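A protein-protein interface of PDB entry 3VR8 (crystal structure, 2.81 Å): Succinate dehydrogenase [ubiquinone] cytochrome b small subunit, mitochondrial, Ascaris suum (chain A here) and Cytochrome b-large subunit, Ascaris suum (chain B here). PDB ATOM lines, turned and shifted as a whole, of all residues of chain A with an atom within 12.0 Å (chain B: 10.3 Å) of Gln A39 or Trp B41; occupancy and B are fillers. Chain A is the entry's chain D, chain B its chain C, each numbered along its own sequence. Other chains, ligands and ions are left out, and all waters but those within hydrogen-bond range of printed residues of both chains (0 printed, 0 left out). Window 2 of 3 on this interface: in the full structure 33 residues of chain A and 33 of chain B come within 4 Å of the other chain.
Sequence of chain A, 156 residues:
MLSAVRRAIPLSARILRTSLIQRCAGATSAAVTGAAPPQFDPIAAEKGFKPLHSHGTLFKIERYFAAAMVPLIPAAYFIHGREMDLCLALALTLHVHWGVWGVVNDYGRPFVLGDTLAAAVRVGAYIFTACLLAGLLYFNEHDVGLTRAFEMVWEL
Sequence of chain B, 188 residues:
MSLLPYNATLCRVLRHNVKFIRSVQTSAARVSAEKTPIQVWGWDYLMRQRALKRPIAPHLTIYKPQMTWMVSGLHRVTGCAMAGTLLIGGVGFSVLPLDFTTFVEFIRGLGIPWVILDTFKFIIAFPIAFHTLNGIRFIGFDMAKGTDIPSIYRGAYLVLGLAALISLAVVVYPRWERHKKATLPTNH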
ATOM      1  N   ALA A  35      -2.192   5.857  -4.917  1.00  0.00           N
ATOM      2  CA  ALA A  35      -2.047   6.040  -3.463  1.00  0.00           C
ATOM      3  C   ALA A  35      -2.415   4.796  -2.651  1.00  0.00           C
ATOM      4  O   ALA A  35      -2.935   3.794  -3.189  1.00  0.00           O
ATOM      5  CB  ALA A  35      -2.864   7.254  -2.977  1.00  0.00           C
ATOM      6  N   ALA A  36      -2.126   4.888  -1.352  1.00  0.00           N
ATOM      7  CA  ALA A  36      -2.393   3.828  -0.374  1.00  0.00           C
ATOM      8  C   ALA A  36      -3.872   3.466  -0.364  1.00  0.00           C
ATOM      9  O   ALA A  36      -4.719   4.360  -0.417  1.00  0.00           O
ATOM     10  CB  ALA A  36      -1.948   4.268   1.021  1.00  0.00           C
ATOM     11  N   PRO A  37      -4.191   2.160  -0.294  1.00  0.00           N
ATOM     12  CA  PRO A  37      -5.592   1.787  -0.367  1.00  0.00           C
ATOM     13  C   PRO A  37      -6.339   2.233   0.899  1.00  0.00           C
ATOM     14  O   PRO A  37      -5.723   2.326   1.968  1.00  0.00           O
ATOM     15  CB  PRO A  37      -5.536   0.265  -0.488  1.00  0.00           C
ATOM     16  CG  PRO A  37      -4.284  -0.119   0.209  1.00  0.00           C
ATOM     17  CD  PRO A  37      -3.321   0.994  -0.049  1.00  0.00           C
ATOM     18  N   PRO A  38      -7.641   2.567   0.769  1.00  0.00           N
ATOM     19  CA  PRO A  38      -8.458   2.939   1.917  1.00  0.00           C
ATOM     20  C   PRO A  38      -8.252   1.924   3.013  1.00  0.00           C
ATOM     21  O   PRO A  38      -8.435   0.739   2.788  1.00  0.00           O
ATOM     22  CB  PRO A  38      -9.886   2.847   1.376  1.00  0.00           C
ATOM     23  CG  PRO A  38      -9.763   2.379  -0.074  1.00  0.00           C
ATOM     24  CD  PRO A  38      -8.392   2.705  -0.490  1.00  0.00           C
ATOM     25  N   GLN A  39      -7.842   2.382   4.182  1.00  0.00           N
ATOM     26  CA  GLN A  39      -7.430   1.486   5.255  1.00  0.00           C
ATOM     27  C   GLN A  39      -7.517   2.230   6.567  1.00  0.00           C
ATOM     28  O   GLN A  39      -7.105   3.381   6.653  1.00  0.00           O
ATOM     29  CB  GLN A  39      -5.993   1.011   5.014  1.00  0.00           C
ATOM     30  CG  GLN A  39      -5.320   0.295   6.185  1.00  0.00           C
ATOM     31  CD  GLN A  39      -3.967  -0.294   5.810  1.00  0.00           C
ATOM     32  OE1 GLN A  39      -3.617  -0.390   4.632  1.00  0.00           O
ATOM     33  NE2 GLN A  39      -3.200  -0.689   6.812  1.00  0.00           N
ATOM     34  N   PHE A  40      -8.053   1.586   7.590  1.00  0.00           N
ATOM     35  CA  PHE A  40      -8.231   2.266   8.856  1.00  0.00           C
ATOM     36  C   PHE A  40      -7.003   2.072   9.727  1.00  0.00           C
ATOM     37  O   PHE A  40      -6.517   0.960   9.878  1.00  0.00           O
ATOM     38  CB  PHE A  40      -9.492   1.763   9.524  1.00  0.00           C
ATOM     39  CG  PHE A  40      -9.909   2.554  10.713  1.00  0.00           C
ATOM     40  CD1 PHE A  40     -10.454   3.818  10.563  1.00  0.00           C
ATOM     41  CD2 PHE A  40      -9.795   2.012  11.991  1.00  0.00           C
ATOM     42  CE1 PHE A  40     -10.857   4.546  11.679  1.00  0.00           C
ATOM     43  CE2 PHE A  40     -10.198   2.730  13.109  1.00  0.00           C
ATOM     44  CZ  PHE A  40     -10.728   4.000  12.955  1.00  0.00           C
ATOM     45  N   ASP A  41      -6.487   3.174  10.262  1.00  0.00           N
ATOM     46  CA  ASP A  41      -5.263   3.173  11.054  1.00  0.00           C
ATOM     47  C   ASP A  41      -5.596   3.555  12.487  1.00  0.00           C
ATOM     48  O   ASP A  41      -5.639   4.737  12.804  1.00  0.00           O
ATOM     49  CB  ASP A  41      -4.253   4.163  10.457  1.00  0.00           C
ATOM     50  CG  ASP A  41      -2.824   3.962  10.995  1.00  0.00           C
ATOM     51  OD1 ASP A  41      -2.606   4.160  12.222  1.00  0.00           O
ATOM     52  OD2 ASP A  41      -1.922   3.619  10.174  1.00  0.00           O
ATOM     53  N   PRO A  42      -5.802   2.558  13.362  1.00  0.00           N
ATOM     54  CA  PRO A  42      -6.509   2.770  14.616  1.00  0.00           C
ATOM     55  C   PRO A  42      -5.753   3.570  15.643  1.00  0.00           C
ATOM     56  O   PRO A  42      -6.347   3.897  16.663  1.00  0.00           O
ATOM     57  CB  PRO A  42      -6.712   1.359  15.140  1.00  0.00           C
ATOM     58  CG  PRO A  42      -5.525   0.660  14.668  1.00  0.00           C
ATOM     59  CD  PRO A  42      -5.217   1.215  13.305  1.00  0.00           C
ATOM     60  N   ILE A  43      -4.469   3.855  15.399  1.00  0.00           N
ATOM     61  CA  ILE A  43      -3.665   4.741  16.277  1.00  0.00           C
ATOM     62  C   ILE A  43      -3.780   6.210  15.837  1.00  0.00           C
ATOM     63  O   ILE A  43      -4.138   7.091  16.632  1.00  0.00           O
ATOM     64  CB  ILE A  43      -2.151   4.355  16.308  1.00  0.00           C
ATOM     65  CG1 ILE A  43      -1.948   2.916  16.784  1.00  0.00           C
ATOM     66  CG2 ILE A  43      -1.350   5.339  17.188  1.00  0.00           C
ATOM     67  CD1 ILE A  43      -0.500   2.436  16.686  1.00  0.00           C
ATOM     68  N   ALA A  44      -3.453   6.439  14.564  1.00  0.00           N
ATOM     69  CA  ALA A  44      -3.507   7.749  13.922  1.00  0.00           C
ATOM     70  C   ALA A  44      -4.884   8.424  14.021  1.00  0.00           C
ATOM     71  O   ALA A  44      -4.977   9.596  14.392  1.00  0.00           O
ATOM     72  CB  ALA A  44      -3.054   7.639  12.462  1.00  0.00           C
ATOM     73  N   ALA A  45      -5.950   7.696  13.696  1.00  0.00           N
ATOM     74  CA  ALA A  45      -7.297   8.258  13.797  1.00  0.00           C
ATOM     75  C   ALA A  45      -7.728   8.430  15.269  1.00  0.00           C
ATOM     76  O   ALA A  45      -8.616   9.241  15.576  1.00  0.00           O
ATOM     77  CB  ALA A  45      -8.303   7.423  12.988  1.00  0.00           C
ATOM     78  N   GLU A  46      -7.064   7.688  16.161  1.00  0.00           N
ATOM     79  CA  GLU A  46      -7.264   7.782  17.611  1.00  0.00           C
ATOM     80  C   GLU A  46      -6.843   9.139  18.219  1.00  0.00           C
ATOM     81  O   GLU A  46      -7.361   9.521  19.276  1.00  0.00           O
ATOM     82  CB  GLU A  46      -6.512   6.628  18.299  1.00  0.00           C
ATOM     83  CG  GLU A  46      -6.445   6.622  19.852  1.00  0.00           C
ATOM     84  CD  GLU A  46      -5.104   6.063  20.383  1.00  0.00           C
ATOM     85  OE1 GLU A  46      -4.919   4.823  20.427  1.00  0.00           O
ATOM     86  OE2 GLU A  46      -4.227   6.872  20.760  1.00  0.00           O
ATOM     87  N   PHE A  49      -9.473  12.692  18.846  1.00  0.00           N
ATOM     88  CA  PHE A  49     -10.788  12.011  18.816  1.00  0.00           C
ATOM     89  C   PHE A  49     -10.924  11.139  20.101  1.00  0.00           C
ATOM     90  O   PHE A  49     -11.173   9.916  20.042  1.00  0.00           O
ATOM     91  CB  PHE A  49     -10.904  11.138  17.547  1.00  0.00           C
ATOM     92  CG  PHE A  49     -11.949  11.604  16.528  1.00  0.00           C
ATOM     93  CD1 PHE A  49     -13.286  11.852  16.909  1.00  0.00           C
ATOM     94  CD2 PHE A  49     -11.611  11.707  15.165  1.00  0.00           C
ATOM     95  CE1 PHE A  49     -14.261  12.245  15.944  1.00  0.00           C
ATOM     96  CE2 PHE A  49     -12.576  12.094  14.196  1.00  0.00           C
ATOM     97  CZ  PHE A  49     -13.898  12.364  14.588  1.00  0.00           C
ATOM     98  N   PHE A 111     -28.360   6.319   5.163  1.00  0.00           N
ATOM     99  CA  PHE A 111     -27.915   5.655   3.923  1.00  0.00           C
ATOM    100  C   PHE A 111     -29.054   5.547   2.917  1.00  0.00           C
ATOM    101  O   PHE A 111     -28.878   5.851   1.740  1.00  0.00           O
ATOM    102  CB  PHE A 111     -27.341   4.270   4.197  1.00  0.00           C
ATOM    103  CG  PHE A 111     -26.741   3.591   2.977  1.00  0.00           C
ATOM    104  CD1 PHE A 111     -25.414   3.843   2.596  1.00  0.00           C
ATOM    105  CD2 PHE A 111     -27.491   2.672   2.227  1.00  0.00           C
ATOM    106  CE1 PHE A 111     -24.835   3.194   1.478  1.00  0.00           C
ATOM    107  CE2 PHE A 111     -26.934   2.029   1.109  1.00  0.00           C
ATOM    108  CZ  PHE A 111     -25.595   2.293   0.738  1.00  0.00           C
ATOM    109  N   LYS B  35     -19.761  10.780  15.676  1.00  0.00           N
ATOM    110  CA  LYS B  35     -19.371   9.482  15.205  1.00  0.00           C
ATOM    111  C   LYS B  35     -17.948   9.273  15.670  1.00  0.00           C
ATOM    112  O   LYS B  35     -17.169  10.226  15.716  1.00  0.00           O
ATOM    113  CB  LYS B  35     -19.555   9.382  13.672  1.00  0.00           C
ATOM    114  CG  LYS B  35     -20.996   9.770  13.192  1.00  0.00           C
ATOM    115  CD  LYS B  35     -21.491   9.151  11.870  1.00  0.00           C
ATOM    116  CE  LYS B  35     -20.793   9.808  10.688  1.00  0.00           C
ATOM    117  NZ  LYS B  35     -21.474   9.630   9.369  1.00  0.00           N
ATOM    118  N   THR B  36     -17.634   8.040  16.075  1.00  0.00           N
ATOM    119  CA  THR B  36     -16.264   7.628  16.407  1.00  0.00           C
ATOM    120  C   THR B  36     -15.408   7.604  15.139  1.00  0.00           C
ATOM    121  O   THR B  36     -15.940   7.709  14.029  1.00  0.00           O
ATOM    122  CB  THR B  36     -16.231   6.250  17.094  1.00  0.00           C
ATOM    123  OG1 THR B  36     -17.230   5.390  16.522  1.00  0.00           O
ATOM    124  CG2 THR B  36     -16.487   6.402  18.582  1.00  0.00           C
ATOM    125  N   PRO B  37     -14.080   7.476  15.275  1.00  0.00           N
ATOM    126  CA  PRO B  37     -13.350   7.545  14.000  1.00  0.00           C
ATOM    127  C   PRO B  37     -13.731   6.432  13.014  1.00  0.00           C
ATOM    128  O   PRO B  37     -13.875   6.712  11.828  1.00  0.00           O
ATOM    129  CB  PRO B  37     -11.880   7.483  14.422  1.00  0.00           C
ATOM    130  CG  PRO B  37     -11.879   7.948  15.853  1.00  0.00           C
ATOM    131  CD  PRO B  37     -13.182   7.474  16.442  1.00  0.00           C
ATOM    132  N   ILE B  38     -13.928   5.207  13.513  1.00  0.00           N
ATOM    133  CA  ILE B  38     -14.452   4.080  12.718  1.00  0.00           C
ATOM    134  C   ILE B  38     -15.862   4.324  12.122  1.00  0.00           C
ATOM    135  O   ILE B  38     -16.080   4.021  10.952  1.00  0.00           O
ATOM    136  CB  ILE B  38     -14.373   2.705  13.499  1.00  0.00           C
ATOM    137  CG1 ILE B  38     -14.573   1.500  12.572  1.00  0.00           C
ATOM    138  CG2 ILE B  38     -15.375   2.643  14.658  1.00  0.00           C
ATOM    139  CD1 ILE B  38     -13.493   1.322  11.540  1.00  0.00           C
ATOM    140  N   GLN B  39     -16.800   4.868  12.901  1.00  0.00           N
ATOM    141  CA  GLN B  39     -18.131   5.230  12.402  1.00  0.00           C
ATOM    142  C   GLN B  39     -18.052   6.168  11.166  1.00  0.00           C
ATOM    143  O   GLN B  39     -18.945   6.146  10.267  1.00  0.00           O
ATOM    144  CB  GLN B  39     -18.971   5.859  13.523  1.00  0.00           C
ATOM    145  CG  GLN B  39     -19.813   4.849  14.299  1.00  0.00           C
ATOM    146  CD  GLN B  39     -20.253   5.274  15.738  1.00  0.00           C
ATOM    147  OE1 GLN B  39     -19.838   6.306  16.265  1.00  0.00           O
ATOM    148  NE2 GLN B  39     -21.098   4.448  16.362  1.00  0.00           N
ATOM    149  N   VAL B  40     -16.988   6.986  11.135  1.00  0.00           N
ATOM    150  CA  VAL B  40     -16.799   7.937  10.059  1.00  0.00           C
ATOM    151  C   VAL B  40     -16.293   7.130   8.910  1.00  0.00           C
ATOM    152  O   VAL B  40     -16.948   7.064   7.868  1.00  0.00           O
ATOM    153  CB  VAL B  40     -15.778   9.049  10.357  1.00  0.00           C
ATOM    154  CG1 VAL B  40     -15.683  10.000   9.157  1.00  0.00           C
ATOM    155  CG2 VAL B  40     -16.163   9.812  11.586  1.00  0.00           C
ATOM    156  N   TRP B  41     -15.135   6.499   9.111  1.00  0.00           N
ATOM    157  CA  TRP B  41     -14.534   5.629   8.096  1.00  0.00           C
ATOM    158  C   TRP B  41     -15.606   4.790   7.414  1.00  0.00           C
ATOM    159  O   TRP B  41     -15.630   4.676   6.181  1.00  0.00           O
ATOM    160  CB  TRP B  41     -13.482   4.698   8.715  1.00  0.00           C
ATOM    161  CG  TRP B  41     -12.656   4.035   7.686  1.00  0.00           C
ATOM    162  CD1 TRP B  41     -11.485   4.471   7.200  1.00  0.00           C
ATOM    163  CD2 TRP B  41     -12.963   2.821   6.978  1.00  0.00           C
ATOM    164  NE1 TRP B  41     -11.023   3.617   6.242  1.00  0.00           N
ATOM    165  CE2 TRP B  41     -11.917   2.591   6.089  1.00  0.00           C
ATOM    166  CE3 TRP B  41     -14.026   1.896   7.025  1.00  0.00           C
ATOM    167  CZ2 TRP B  41     -11.890   1.476   5.245  1.00  0.00           C
ATOM    168  CZ3 TRP B  41     -14.003   0.794   6.181  1.00  0.00           C
ATOM    169  CH2 TRP B  41     -12.946   0.600   5.306  1.00  0.00           C
ATOM    170  N   GLY B  42     -16.486   4.230   8.246  1.00  0.00           N
ATOM    171  CA  GLY B  42     -17.544   3.336   7.830  1.00  0.00           C
ATOM    172  C   GLY B  42     -18.572   3.966   6.918  1.00  0.00           C
ATOM    173  O   GLY B  42     -19.037   3.314   5.977  1.00  0.00           O
ATOM    174  N   TRP B  43     -18.941   5.221   7.185  1.00  0.00           N
ATOM    175  CA  TRP B  43     -19.859   5.914   6.283  1.00  0.00           C
ATOM    176  C   TRP B  43     -19.192   6.113   4.914  1.00  0.00           C
ATOM    177  O   TRP B  43     -19.736   5.695   3.891  1.00  0.00           O
ATOM    178  CB  TRP B  43     -20.408   7.224   6.869  1.00  0.00           C
ATOM    179  CG  TRP B  43     -21.237   7.974   5.873  1.00  0.00           C
ATOM    180  CD1 TRP B  43     -20.797   8.941   5.019  1.00  0.00           C
ATOM    181  CD2 TRP B  43     -22.623   7.785   5.576  1.00  0.00           C
ATOM    182  NE1 TRP B  43     -21.825   9.376   4.224  1.00  0.00           N
ATOM    183  CE2 TRP B  43     -22.958   8.684   4.549  1.00  0.00           C
ATOM    184  CE3 TRP B  43     -23.612   6.952   6.082  1.00  0.00           C
ATOM    185  CZ2 TRP B  43     -24.235   8.782   4.030  1.00  0.00           C
ATOM    186  CZ3 TRP B  43     -24.895   7.046   5.547  1.00  0.00           C
ATOM    187  CH2 TRP B  43     -25.186   7.952   4.529  1.00  0.00           C
ATOM    188  N   ASP B  44     -18.000   6.703   4.893  1.00  0.00           N
ATOM    189  CA  ASP B  44     -17.258   6.821   3.636  1.00  0.00           C
ATOM    190  C   ASP B  44     -17.182   5.481   2.914  1.00  0.00           C
ATOM    191  O   ASP B  44     -17.243   5.455   1.676  1.00  0.00           O
ATOM    192  CB  ASP B  44     -15.850   7.361   3.861  1.00  0.00           C
ATOM    193  CG  ASP B  44     -15.848   8.711   4.538  1.00  0.00           C
ATOM    194  OD1 ASP B  44     -14.749   9.183   4.912  1.00  0.00           O
ATOM    195  OD2 ASP B  44     -16.940   9.303   4.700  1.00  0.00           O
ATOM    196  N   TYR B  45     -17.055   4.389   3.685  1.00  0.00           N
ATOM    197  CA  TYR B  45     -17.022   3.035   3.131  1.00  0.00           C
ATOM    198  C   TYR B  45     -18.298   2.787   2.378  1.00  0.00           C
ATOM    199  O   TYR B  45     -18.259   2.366   1.232  1.00  0.00           O
ATOM    200  CB  TYR B  45     -16.865   1.954   4.209  1.00  0.00           C
ATOM    201  CG  TYR B  45     -17.130   0.558   3.680  1.00  0.00           C
ATOM    202  CD1 TYR B  45     -16.128  -0.170   3.037  1.00  0.00           C
ATOM    203  CD2 TYR B  45     -18.389  -0.033   3.803  1.00  0.00           C
ATOM    204  CE1 TYR B  45     -16.379  -1.464   2.534  1.00  0.00           C
ATOM    205  CE2 TYR B  45     -18.646  -1.309   3.293  1.00  0.00           C
ATOM    206  CZ  TYR B  45     -17.638  -2.008   2.666  1.00  0.00           C
ATOM    207  OH  TYR B  45     -17.887  -3.253   2.185  1.00  0.00           O
ATOM    208  N   LEU B  46     -19.421   3.040   3.042  1.00  0.00           N
ATOM    209  CA  LEU B  46     -20.715   2.896   2.412  1.00  0.00           C
ATOM    210  C   LEU B  46     -20.837   3.736   1.110  1.00  0.00           C
ATOM    211  O   LEU B  46     -21.227   3.231   0.048  1.00  0.00           O
ATOM    212  CB  LEU B  46     -21.810   3.271   3.398  1.00  0.00           C
ATOM    213  CG  LEU B  46     -22.289   2.254   4.410  1.00  0.00           C
ATOM    214  CD1 LEU B  46     -23.493   2.816   5.102  1.00  0.00           C
ATOM    215  CD2 LEU B  46     -22.651   0.951   3.761  1.00  0.00           C
ATOM    216  N   MET B  47     -20.479   5.013   1.203  1.00  0.00           N
ATOM    217  CA  MET B  47     -20.497   5.927   0.064  1.00  0.00           C
ATOM    218  C   MET B  47     -19.633   5.440  -1.098  1.00  0.00           C
ATOM    219  O   MET B  47     -20.046   5.544  -2.272  1.00  0.00           O
ATOM    220  CB  MET B  47     -20.063   7.332   0.502  1.00  0.00           C
ATOM    221  CG  MET B  47     -21.078   8.050   1.355  1.00  0.00           C
ATOM    222  SD  MET B  47     -22.678   7.829   0.581  1.00  0.00           S
ATOM    223  CE  MET B  47     -23.437   6.559   1.602  1.00  0.00           C
ATOM    224  N   ARG B  48     -18.439   4.929  -0.758  1.00  0.00           N
ATOM    225  CA  ARG B  48     -17.558   4.263  -1.719  1.00  0.00           C
ATOM    226  C   ARG B  48     -18.357   3.158  -2.398  1.00  0.00           C
ATOM    227  O   ARG B  48     -18.527   3.170  -3.620  1.00  0.00           O
ATOM    228  CB  ARG B  48     -16.320   3.661  -1.029  1.00  0.00           C
ATOM    229  CG  ARG B  48     -15.012   4.425  -1.181  1.00  0.00           C
ATOM    230  CD  ARG B  48     -13.915   3.716  -0.412  1.00  0.00           C
ATOM    231  NE  ARG B  48     -13.832   4.171   0.982  1.00  0.00           N
ATOM    232  CZ  ARG B  48     -13.519   3.398   2.037  1.00  0.00           C
ATOM    233  NH1 ARG B  48     -13.272   2.090   1.880  1.00  0.00           N
ATOM    234  NH2 ARG B  48     -13.463   3.926   3.268  1.00  0.00           N
ATOM    235  N   GLN B  49     -18.887   2.240  -1.593  1.00  0.00           N
ATOM    236  CA  GLN B  49     -19.455   1.011  -2.109  1.00  0.00           C
ATOM    237  C   GLN B  49     -20.727   1.333  -2.836  1.00  0.00           C
ATOM    238  O   GLN B  49     -21.173   0.561  -3.686  1.00  0.00           O
ATOM    239  CB  GLN B  49     -19.710  -0.016  -0.988  1.00  0.00           C
ATOM    240  CG  GLN B  49     -18.458  -0.497  -0.240  1.00  0.00           C
ATOM    241  CD  GLN B  49     -17.541  -1.349  -1.093  1.00  0.00           C
ATOM    242  OE1 GLN B  49     -17.986  -2.058  -1.993  1.00  0.00           O
ATOM    243  NE2 GLN B  49     -16.254  -1.298  -0.804  1.00  0.00           N
ATOM    244  N   ARG B  54     -22.159  -1.741  -6.475  1.00  0.00           N
ATOM    245  CA  ARG B  54     -22.200  -3.153  -6.162  1.00  0.00           C
ATOM    246  C   ARG B  54     -23.534  -3.478  -5.511  1.00  0.00           C
ATOM    247  O   ARG B  54     -23.968  -2.738  -4.636  1.00  0.00           O
ATOM    248  CB  ARG B  54     -21.059  -3.505  -5.216  1.00  0.00           C
ATOM    249  CG  ARG B  54     -19.678  -3.219  -5.784  1.00  0.00           C
ATOM    250  CD  ARG B  54     -18.614  -3.583  -4.807  1.00  0.00           C
ATOM    251  NE  ARG B  54     -17.359  -3.800  -5.491  1.00  0.00           N
ATOM    252  CZ  ARG B  54     -16.180  -3.584  -4.933  1.00  0.00           C
ATOM    253  NH1 ARG B  54     -16.113  -3.138  -3.687  1.00  0.00           N
ATOM    254  NH2 ARG B  54     -15.073  -3.800  -5.626  1.00  0.00           N
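Trp B41 touches Gln A39 (NE1 to C, 3.8 Å). Phe A40 touches Pro B37. Ile B38 touches Phe A40. CD1 of Phe A40 touches CD1 of Trp B41 (3.6 Å). O of Ala A45 touches CG of Pro B37 (3.5 Å). O of Lys B35 touches CE1 of Phe A49 (3.5 Å). CG of Phe A49 touches CG of Pro B37, at 3.7 Å. Phe A111 touches Trp B43. Phe A111 touches Leu B46 (CD1 to CD1, 3.3 Å). Met B47 touches Phe A111 (CE to CD1, 3.5 Å).
Gln A39 touches just one residue of chain B: Trp B41 (3.8 Å). Phe A40 touches three residues of chain B. Printed residues of chain B within 4 Å of Phe A49: Lys B35 (3.5 Å) and Pro B37 (3.7 Å). Printed residues of chain A within 4 Å of Lys B35: Phe A49. Of chain A, only Phe A40, Ala A45 and Phe A49 come within 4 Å of Pro B37. Printed residues of chain A within 4 Å of Ile B38: Phe A40 (3.5 Å). No residue of chain A comes within 4 Å of Val B40. Of chain A, only Gln A39 and Phe A40 come within 4 Å of Trp B41. No residue of chain A comes within 4 Å of Gly B42. No residue of chain A comes within 4 Å of Asp B44. Tyr B45 touches none of the printed residues of chain A. Printed residues of chain A within 4 Å of Leu B46: Phe A111 (3.3 Å). Printed residues of chain A within 4 Å of Arg B48: Pro A38. The nearest residue of chain B that does not touch Gln A39 is Arg B48 (5.9 Å).
Of the 14 printed residues of chain A, 6 touch a printed residue of chain B. Hydrophobic or aromatic side chains of chain B that line the printed part of chain A: Pro B37, Ile B38, Trp B41, Trp B43, Leu B46 and Met B47. Among the printed residues, no Asp or Glu carboxylate lies within 4 Å of a Lys or Arg side-chain nitrogen of the other chain.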
